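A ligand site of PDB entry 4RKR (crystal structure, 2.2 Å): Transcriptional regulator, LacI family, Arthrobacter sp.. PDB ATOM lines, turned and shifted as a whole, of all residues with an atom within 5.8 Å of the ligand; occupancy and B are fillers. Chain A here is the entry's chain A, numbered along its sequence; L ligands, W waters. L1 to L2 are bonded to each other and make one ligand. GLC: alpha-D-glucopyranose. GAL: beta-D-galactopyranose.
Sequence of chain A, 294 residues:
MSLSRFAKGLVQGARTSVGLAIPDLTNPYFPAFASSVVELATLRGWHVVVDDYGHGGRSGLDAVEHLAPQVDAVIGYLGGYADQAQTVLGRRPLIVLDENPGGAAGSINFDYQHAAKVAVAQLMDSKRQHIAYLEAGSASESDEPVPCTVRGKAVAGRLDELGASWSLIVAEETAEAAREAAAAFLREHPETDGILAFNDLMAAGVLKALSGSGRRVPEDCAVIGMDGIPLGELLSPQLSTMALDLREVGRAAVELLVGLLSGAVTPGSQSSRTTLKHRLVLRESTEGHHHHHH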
ATOM      1  N   PRO A  23      14.734 -11.193  -1.885  1.00  0.00           N
ATOM      2  CA  PRO A  23      15.269 -11.408  -3.228  1.00  0.00           C
ATOM      3  C   PRO A  23      14.252 -11.364  -4.377  1.00  0.00           C
ATOM      4  O   PRO A  23      14.639 -11.195  -5.518  1.00  0.00           O
ATOM      5  CB  PRO A  23      15.900 -12.790  -3.138  1.00  0.00           C
ATOM      6  CG  PRO A  23      15.144 -13.481  -2.052  1.00  0.00           C
ATOM      7  CD  PRO A  23      14.824 -12.408  -1.053  1.00  0.00           C
ATOM      8  N   ASN A  27       8.049 -15.513  -5.581  1.00  0.00           N
ATOM      9  CA  ASN A  27       7.905 -16.756  -4.791  1.00  0.00           C
ATOM     10  C   ASN A  27       7.044 -16.418  -3.574  1.00  0.00           C
ATOM     11  O   ASN A  27       7.510 -15.694  -2.714  1.00  0.00           O
ATOM     12  CB  ASN A  27       9.271 -17.298  -4.378  1.00  0.00           C
ATOM     13  CG  ASN A  27       9.193 -18.446  -3.364  1.00  0.00           C
ATOM     14  OD1 ASN A  27       8.113 -18.904  -2.989  1.00  0.00           O
ATOM     15  ND2 ASN A  27      10.349 -18.929  -2.951  1.00  0.00           N
ATOM     16  N   TYR A  29       6.407 -17.355  -0.799  1.00  0.00           N
ATOM     17  CA  TYR A  29       7.040 -17.372   0.510  1.00  0.00           C
ATOM     18  C   TYR A  29       7.426 -15.968   0.978  1.00  0.00           C
ATOM     19  O   TYR A  29       7.179 -15.598   2.127  1.00  0.00           O
ATOM     20  CB  TYR A  29       8.274 -18.267   0.541  1.00  0.00           C
ATOM     21  CG  TYR A  29       9.009 -18.170   1.856  1.00  0.00           C
ATOM     22  CD1 TYR A  29       8.544 -18.846   2.989  1.00  0.00           C
ATOM     23  CD2 TYR A  29      10.144 -17.362   1.984  1.00  0.00           C
ATOM     24  CE1 TYR A  29       9.194 -18.732   4.211  1.00  0.00           C
ATOM     25  CE2 TYR A  29      10.799 -17.240   3.207  1.00  0.00           C
ATOM     26  CZ  TYR A  29      10.324 -17.929   4.315  1.00  0.00           C
ATOM     27  OH  TYR A  29      10.971 -17.811   5.523  1.00  0.00           O
ATOM     28  N   PHE A  30       8.038 -15.181   0.113  1.00  0.00           N
ATOM     29  CA  PHE A  30       8.599 -13.909   0.577  1.00  0.00           C
ATOM     30  C   PHE A  30       7.564 -12.854   0.928  1.00  0.00           C
ATOM     31  O   PHE A  30       7.706 -12.185   1.930  1.00  0.00           O
ATOM     32  CB  PHE A  30       9.634 -13.381  -0.399  1.00  0.00           C
ATOM     33  CG  PHE A  30      10.840 -14.266  -0.501  1.00  0.00           C
ATOM     34  CD1 PHE A  30      11.708 -14.409   0.575  1.00  0.00           C
ATOM     35  CD2 PHE A  30      11.094 -14.994  -1.654  1.00  0.00           C
ATOM     36  CE1 PHE A  30      12.798 -15.236   0.491  1.00  0.00           C
ATOM     37  CE2 PHE A  30      12.193 -15.814  -1.746  1.00  0.00           C
ATOM     38  CZ  PHE A  30      13.047 -15.937  -0.667  1.00  0.00           C
ATOM     39  N   TYR A  53      14.962  -6.898  -4.178  1.00  0.00           N
ATOM     40  CA  TYR A  53      16.123  -6.701  -5.021  1.00  0.00           C
ATOM     41  C   TYR A  53      16.245  -7.676  -6.195  1.00  0.00           C
ATOM     42  O   TYR A  53      17.269  -7.714  -6.856  1.00  0.00           O
ATOM     43  CB  TYR A  53      17.386  -6.715  -4.175  1.00  0.00           C
ATOM     44  CG  TYR A  53      17.725  -8.002  -3.434  1.00  0.00           C
ATOM     45  CD1 TYR A  53      18.469  -8.986  -4.042  1.00  0.00           C
ATOM     46  CD2 TYR A  53      17.401  -8.164  -2.102  1.00  0.00           C
ATOM     47  CE1 TYR A  53      18.831 -10.136  -3.365  1.00  0.00           C
ATOM     48  CE2 TYR A  53      17.746  -9.317  -1.421  1.00  0.00           C
ATOM     49  CZ  TYR A  53      18.470 -10.295  -2.060  1.00  0.00           C
ATOM     50  OH  TYR A  53      18.849 -11.441  -1.409  1.00  0.00           O
ATOM     51  N   TYR A  77      16.880 -11.780   3.639  1.00  0.00           N
ATOM     52  CA  TYR A  77      17.502 -12.845   2.880  1.00  0.00           C
ATOM     53  C   TYR A  77      18.475 -12.163   1.922  1.00  0.00           C
ATOM     54  O   TYR A  77      18.072 -11.389   1.059  1.00  0.00           O
ATOM     55  CB  TYR A  77      16.432 -13.623   2.117  1.00  0.00           C
ATOM     56  CG  TYR A  77      15.659 -14.603   2.961  1.00  0.00           C
ATOM     57  CD1 TYR A  77      14.582 -14.185   3.766  1.00  0.00           C
ATOM     58  CD2 TYR A  77      15.960 -15.956   2.937  1.00  0.00           C
ATOM     59  CE1 TYR A  77      13.864 -15.093   4.524  1.00  0.00           C
ATOM     60  CE2 TYR A  77      15.249 -16.870   3.699  1.00  0.00           C
ATOM     61  CZ  TYR A  77      14.204 -16.431   4.471  1.00  0.00           C
ATOM     62  OH  TYR A  77      13.539 -17.337   5.230  1.00  0.00           O
ATOM     63  N   GLY A  79      21.133 -13.573  -0.039  1.00  0.00           N
ATOM     64  CA  GLY A  79      21.722 -14.324  -1.153  1.00  0.00           C
ATOM     65  C   GLY A  79      23.224 -14.546  -1.032  1.00  0.00           C
ATOM     66  O   GLY A  79      23.928 -14.568  -2.020  1.00  0.00           O
ATOM     67  N   LEU A  97      18.600 -14.474   7.380  1.00  0.00           N
ATOM     68  CA  LEU A  97      17.901 -15.766   7.452  1.00  0.00           C
ATOM     69  C   LEU A  97      18.485 -16.770   6.492  1.00  0.00           C
ATOM     70  O   LEU A  97      18.939 -16.435   5.391  1.00  0.00           O
ATOM     71  CB  LEU A  97      16.409 -15.613   7.170  1.00  0.00           C
ATOM     72  CG  LEU A  97      15.648 -14.988   8.347  1.00  0.00           C
ATOM     73  CD1 LEU A  97      15.514 -13.487   8.170  1.00  0.00           C
ATOM     74  CD2 LEU A  97      14.290 -15.616   8.526  1.00  0.00           C
ATOM     75  N   ASP A  98      18.509 -18.016   6.959  1.00  0.00           N
ATOM     76  CA  ASP A  98      18.728 -19.164   6.103  1.00  0.00           C
ATOM     77  C   ASP A  98      20.028 -19.107   5.318  1.00  0.00           C
ATOM     78  O   ASP A  98      20.061 -19.535   4.172  1.00  0.00           O
ATOM     79  CB  ASP A  98      17.534 -19.284   5.152  1.00  0.00           C
ATOM     80  CG  ASP A  98      17.299 -20.706   4.653  1.00  0.00           C
ATOM     81  OD1 ASP A  98      17.926 -21.676   5.135  1.00  0.00           O
ATOM     82  OD2 ASP A  98      16.468 -20.820   3.748  1.00  0.00           O
ATOM     83  N   GLU A  99      21.091 -18.564   5.913  1.00  0.00           N
ATOM     84  CA  GLU A  99      22.429 -18.625   5.303  1.00  0.00           C
ATOM     85  C   GLU A  99      23.512 -18.446   6.340  1.00  0.00           C
ATOM     86  O   GLU A  99      23.247 -18.026   7.464  1.00  0.00           O
ATOM     87  CB  GLU A  99      22.598 -17.569   4.198  1.00  0.00           C
ATOM     88  CG  GLU A  99      22.589 -16.123   4.666  1.00  0.00           C
ATOM     89  CD  GLU A  99      22.904 -15.152   3.526  1.00  0.00           C
ATOM     90  OE1 GLU A  99      24.087 -14.852   3.327  1.00  0.00           O
ATOM     91  OE2 GLU A  99      21.971 -14.662   2.824  1.00  0.00           O
ATOM     92  N   PHE A 110      17.249 -22.784   9.969  1.00  0.00           N
ATOM     93  CA  PHE A 110      16.254 -23.819  10.109  1.00  0.00           C
ATOM     94  C   PHE A 110      16.907 -25.186  10.152  1.00  0.00           C
ATOM     95  O   PHE A 110      17.963 -25.417   9.553  1.00  0.00           O
ATOM     96  CB  PHE A 110      15.266 -23.711   8.963  1.00  0.00           C
ATOM     97  CG  PHE A 110      14.675 -22.334   8.815  1.00  0.00           C
ATOM     98  CD1 PHE A 110      13.709 -21.888   9.697  1.00  0.00           C
ATOM     99  CD2 PHE A 110      15.096 -21.494   7.805  1.00  0.00           C
ATOM    100  CE1 PHE A 110      13.167 -20.615   9.573  1.00  0.00           C
ATOM    101  CE2 PHE A 110      14.550 -20.217   7.668  1.00  0.00           C
ATOM    102  CZ  PHE A 110      13.587 -19.784   8.553  1.00  0.00           C
ATOM    103  N   TYR A 112      17.106 -28.358   8.784  1.00  0.00           N
ATOM    104  CA  TYR A 112      16.661 -29.073   7.570  1.00  0.00           C
ATOM    105  C   TYR A 112      16.779 -30.601   7.666  1.00  0.00           C
ATOM    106  O   TYR A 112      16.152 -31.330   6.880  1.00  0.00           O
ATOM    107  CB  TYR A 112      17.401 -28.565   6.327  1.00  0.00           C
ATOM    108  CG  TYR A 112      16.890 -27.206   5.853  1.00  0.00           C
ATOM    109  CD1 TYR A 112      15.567 -27.055   5.424  1.00  0.00           C
ATOM    110  CD2 TYR A 112      17.719 -26.087   5.860  1.00  0.00           C
ATOM    111  CE1 TYR A 112      15.093 -25.823   5.016  1.00  0.00           C
ATOM    112  CE2 TYR A 112      17.236 -24.860   5.438  1.00  0.00           C
ATOM    113  CZ  TYR A 112      15.927 -24.732   5.029  1.00  0.00           C
ATOM    114  OH  TYR A 112      15.436 -23.534   4.608  1.00  0.00           O
ATOM    115  N   VAL A 150      21.094 -27.023   0.750  1.00  0.00           N
ATOM    116  CA  VAL A 150      21.261 -27.524   2.089  1.00  0.00           C
ATOM    117  C   VAL A 150      20.191 -28.539   2.424  1.00  0.00           C
ATOM    118  O   VAL A 150      20.496 -29.647   2.862  1.00  0.00           O
ATOM    119  CB  VAL A 150      21.226 -26.385   3.136  1.00  0.00           C
ATOM    120  CG1 VAL A 150      21.182 -26.956   4.557  1.00  0.00           C
ATOM    121  CG2 VAL A 150      22.444 -25.469   2.944  1.00  0.00           C
ATOM    122  N   ARG A 151      18.928 -28.149   2.241  1.00  0.00           N
ATOM    123  CA  ARG A 151      17.819 -29.080   2.482  1.00  0.00           C
ATOM    124  C   ARG A 151      17.888 -30.247   1.486  1.00  0.00           C
ATOM    125  O   ARG A 151      17.571 -31.385   1.835  1.00  0.00           O
ATOM    126  CB  ARG A 151      16.467 -28.367   2.413  1.00  0.00           C
ATOM    127  CG  ARG A 151      16.060 -27.934   1.013  1.00  0.00           C
ATOM    128  CD  ARG A 151      14.829 -27.048   1.039  1.00  0.00           C
ATOM    129  NE  ARG A 151      15.152 -25.651   1.316  1.00  0.00           N
ATOM    130  CZ  ARG A 151      14.278 -24.647   1.195  1.00  0.00           C
ATOM    131  NH1 ARG A 151      13.026 -24.864   0.804  1.00  0.00           N
ATOM    132  NH2 ARG A 151      14.667 -23.399   1.478  1.00  0.00           N
ATOM    133  N   GLU A 173      13.641 -22.699  -9.783  1.00  0.00           N
ATOM    134  CA  GLU A 173      12.673 -22.559  -8.717  1.00  0.00           C
ATOM    135  C   GLU A 173      11.446 -21.766  -9.170  1.00  0.00           C
ATOM    136  O   GLU A 173      11.205 -20.648  -8.714  1.00  0.00           O
ATOM    137  CB  GLU A 173      13.358 -21.921  -7.508  1.00  0.00           C
ATOM    138  CG  GLU A 173      12.511 -21.799  -6.244  1.00  0.00           C
ATOM    139  CD  GLU A 173      13.279 -21.194  -5.083  1.00  0.00           C
ATOM    140  OE1 GLU A 173      14.523 -21.028  -5.171  1.00  0.00           O
ATOM    141  OE2 GLU A 173      12.637 -20.883  -4.064  1.00  0.00           O
ATOM    142  N   PHE A 198      11.343 -29.212  -3.237  1.00  0.00           N
ATOM    143  CA  PHE A 198      12.168 -28.198  -2.580  1.00  0.00           C
ATOM    144  C   PHE A 198      11.312 -27.220  -1.767  1.00  0.00           C
ATOM    145  O   PHE A 198      11.606 -26.938  -0.602  1.00  0.00           O
ATOM    146  CB  PHE A 198      12.991 -27.459  -3.632  1.00  0.00           C
ATOM    147  CG  PHE A 198      13.776 -26.313  -3.077  1.00  0.00           C
ATOM    148  CD1 PHE A 198      14.994 -26.543  -2.452  1.00  0.00           C
ATOM    149  CD2 PHE A 198      13.310 -25.017  -3.193  1.00  0.00           C
ATOM    150  CE1 PHE A 198      15.734 -25.483  -1.926  1.00  0.00           C
ATOM    151  CE2 PHE A 198      14.037 -23.961  -2.672  1.00  0.00           C
ATOM    152  CZ  PHE A 198      15.259 -24.195  -2.034  1.00  0.00           C
ATOM    153  N   ASN A 199      10.245 -26.719  -2.375  1.00  0.00           N
ATOM    154  CA  ASN A 199       9.327 -25.870  -1.637  1.00  0.00           C
ATOM    155  C   ASN A 199       7.903 -25.921  -2.214  1.00  0.00           C
ATOM    156  O   ASN A 199       7.654 -26.595  -3.218  1.00  0.00           O
ATOM    157  CB  ASN A 199       9.864 -24.434  -1.591  1.00  0.00           C
ATOM    158  CG  ASN A 199       9.966 -23.798  -2.963  1.00  0.00           C
ATOM    159  OD1 ASN A 199       9.459 -24.325  -3.967  1.00  0.00           O
ATOM    160  ND2 ASN A 199      10.631 -22.641  -3.021  1.00  0.00           N
ATOM    161  N   MET A 226       7.482 -27.728   1.049  1.00  0.00           N
ATOM    162  CA  MET A 226       8.092 -27.043   2.163  1.00  0.00           C
ATOM    163  C   MET A 226       7.712 -25.563   2.125  1.00  0.00           C
ATOM    164  O   MET A 226       7.580 -24.989   1.066  1.00  0.00           O
ATOM    165  CB  MET A 226       9.604 -27.226   2.118  1.00  0.00           C
ATOM    166  CG  MET A 226      10.346 -26.656   3.306  1.00  0.00           C
ATOM    167  SD  MET A 226      12.056 -27.216   3.497  1.00  0.00           S
ATOM    168  CE  MET A 226      11.883 -28.955   3.145  1.00  0.00           C
ATOM    169  N   ASP A 227       7.596 -24.984   3.324  1.00  0.00           N
ATOM    170  CA  ASP A 227       7.302 -23.577   3.629  1.00  0.00           C
ATOM    171  C   ASP A 227       5.948 -23.263   4.274  1.00  0.00           C
ATOM    172  O   ASP A 227       5.875 -22.380   5.109  1.00  0.00           O
ATOM    173  CB  ASP A 227       7.404 -22.654   2.404  1.00  0.00           C
ATOM    174  CG  ASP A 227       8.793 -22.574   1.830  1.00  0.00           C
ATOM    175  OD1 ASP A 227       9.725 -23.108   2.428  1.00  0.00           O
ATOM    176  OD2 ASP A 227       8.941 -21.970   0.757  1.00  0.00           O
ATOM    177  N   LEU A 244       6.553 -23.746   8.040  1.00  0.00           N
ATOM    178  CA  LEU A 244       7.099 -22.787   8.979  1.00  0.00           C
ATOM    179  C   LEU A 244       5.978 -21.886   9.468  1.00  0.00           C
ATOM    180  O   LEU A 244       5.197 -21.358   8.651  1.00  0.00           O
ATOM    181  CB  LEU A 244       8.136 -21.896   8.295  1.00  0.00           C
ATOM    182  CG  LEU A 244       9.438 -22.514   7.780  1.00  0.00           C
ATOM    183  CD1 LEU A 244      10.244 -21.472   7.030  1.00  0.00           C
ATOM    184  CD2 LEU A 244      10.230 -23.084   8.948  1.00  0.00           C
HETATM  185  C1  GLC L   1      19.633 -19.276   0.480  1.00  0.00           C
HETATM  186  C2  GLC L   1      18.962 -20.355   1.327  1.00  0.00           C
HETATM  187  C3  GLC L   1      17.710 -20.890   0.649  1.00  0.00           C
HETATM  188  C4  GLC L   1      16.786 -19.733   0.321  1.00  0.00           C
HETATM  189  C5  GLC L   1      17.534 -18.754  -0.577  1.00  0.00           C
HETATM  190  C6  GLC L   1      16.642 -17.576  -0.939  1.00  0.00           C
HETATM  191  O1  GLC L   1      20.216 -19.876  -0.678  1.00  0.00           O
HETATM  192  O2  GLC L   1      19.825 -21.479   1.514  1.00  0.00           O
HETATM  193  O3  GLC L   1      17.072 -21.847   1.493  1.00  0.00           O
HETATM  194  O4  GLC L   1      15.660 -20.248  -0.371  1.00  0.00           O
HETATM  195  O5  GLC L   1      18.724 -18.256   0.045  1.00  0.00           O
HETATM  196  O6  GLC L   1      17.425 -16.548  -1.565  1.00  0.00           O
HETATM  197  C1  GAL L   2      14.415 -19.886   0.205  1.00  0.00           C
HETATM  198  C2  GAL L   2      13.271 -20.417  -0.646  1.00  0.00           C
HETATM  199  C3  GAL L   2      11.921 -20.129   0.004  1.00  0.00           C
HETATM  200  C4  GAL L   2      11.925 -20.591   1.453  1.00  0.00           C
HETATM  201  C5  GAL L   2      13.132 -20.050   2.198  1.00  0.00           C
HETATM  202  C6  GAL L   2      13.180 -20.617   3.604  1.00  0.00           C
HETATM  203  O2  GAL L   2      13.328 -19.777  -1.929  1.00  0.00           O
HETATM  204  O3  GAL L   2      10.839 -20.784  -0.649  1.00  0.00           O
HETATM  205  O4  GAL L   2      11.941 -22.012   1.480  1.00  0.00           O
HETATM  206  O5  GAL L   2      14.349 -20.407   1.533  1.00  0.00           O
HETATM  207  O6  GAL L   2      14.078 -19.829   4.378  1.00  0.00           O
HETATM  208  O   HOH W   1      21.039 -23.845   0.399  1.00  0.00           O
HETATM  209  O   HOH W   2      19.269 -15.575   1.571  1.00  0.00           O
HETATM  210  O   HOH W   3      11.700 -24.044   3.983  1.00  0.00           O
HETATM  211  O   HOH W   4      19.721 -23.331   3.064  1.00  0.00           O
HETATM  212  O   HOH W   5      17.876 -25.220   1.525  1.00  0.00           O
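Water W4 lies within hydrogen-bond range of an oxygen (O2) of GLC L1 and the side-chain carboxylate (OD1) of Asp 98.
Water W1 lies within hydrogen-bond range of O2 of GLC L1 (2.9 Å) and N of Val 150 (3.2 Å).
Water W2 lies within hydrogen-bond range of OE2 of Glu 99 (3.1 Å), O5 of GLC L1 (3.1 Å) and N of Gly 79 (3.2 Å).
Water W3 lies within hydrogen-bond range of the side-chain carboxylate of Asp 227 (2.7 Å), the side-chain sulfur of Met 226 (3.2 Å) and an oxygen (O4) of GAL L2 (3.2 Å).
Water W5 lies within hydrogen-bond range of NE of Arg 151 (2.8 Å) and O3 of GLC L1 (3.5 Å).
CG of Pro 23 touches O6 of GLC L1 (3.9 Å).
CD2 of Tyr 29 touches C4 of GAL L2, at 3.7 Å.
CZ of Phe 30 touches C6 of GLC L1, at 3.96 Å.
CE2 of Phe 110 touches O6 of GAL L2, at 3.3 Å.
OH of Tyr 112 touches C6 of GAL L2 (3.8 Å).
12 residues have an atom within 4 Å of the ligand: Pro 23, Asn 27, Tyr 29, Phe 30, Tyr 77, Asp 98, Phe 110, Tyr 112, Arg 151, Glu 173, Asn 199 and Asp 227.
OD2 of Asp 227 is in hydrogen-bond range of O3 of GAL L2, 2.6 Å away.
O3 of GLC L1 lies within hydrogen-bond range of NH2 of Arg 151, 2.9 Å away.
The side-chain amide nitrogen of Asn 27 sits at hydrogen-bond distance from an oxygen (O3) of GAL L2, 3.0 Å away.
O6 of GAL L2 sits at hydrogen-bond distance from OH of Tyr 77, 2.7 Å away.
O3 of GAL L2 is in hydrogen-bond range of ND2 of Asn 199, 3.0 Å away.
The backbone carbonyl oxygen of Asp 98 sits close to an oxygen (O2) of GLC L1 (3.3 Å).
The side-chain carboxylate (OD2) of Asp 98 sits at hydrogen-bond distance from an oxygen (O3) of GLC L1 (2.6 Å).
O2 of GAL L2 is in hydrogen-bond range of OE2 of Glu 173, 2.5 Å away.
O of Tyr 77 lies within hydrogen-bond range of OH of Tyr 53 (2.6 Å).
The side-chain hydroxyl of Tyr 77 lies within hydrogen-bond range of the side-chain hydroxyl of Tyr 29 (2.6 Å).
The side-chain amide oxygen (OD1) of Asn 27 sits close to the backbone NH (N) of Tyr 29, at 3.2 Å.
The guanidinium group (NH1) of Arg 151 lies within hydrogen-bond range of the backbone carbonyl oxygen (O) of Phe 198, at 2.9 Å.
The guanidinium group of Arg 151 lies within hydrogen-bond range of the side-chain hydroxyl of Tyr 112, 3.2 Å away.
O of Asp 227 sits at hydrogen-bond distance from N of Leu 244 (3.3 Å).
The side-chain carboxylate (OD2) of Asp 98 is in hydrogen-bond range of the side-chain hydroxyl (OH) of Tyr 112 (3.0 Å).
The side-chain carboxylate (OD2) of Asp 98 lies within salt-bridge range of the guanidinium group (NH2) of Arg 151, at 3.9 Å.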
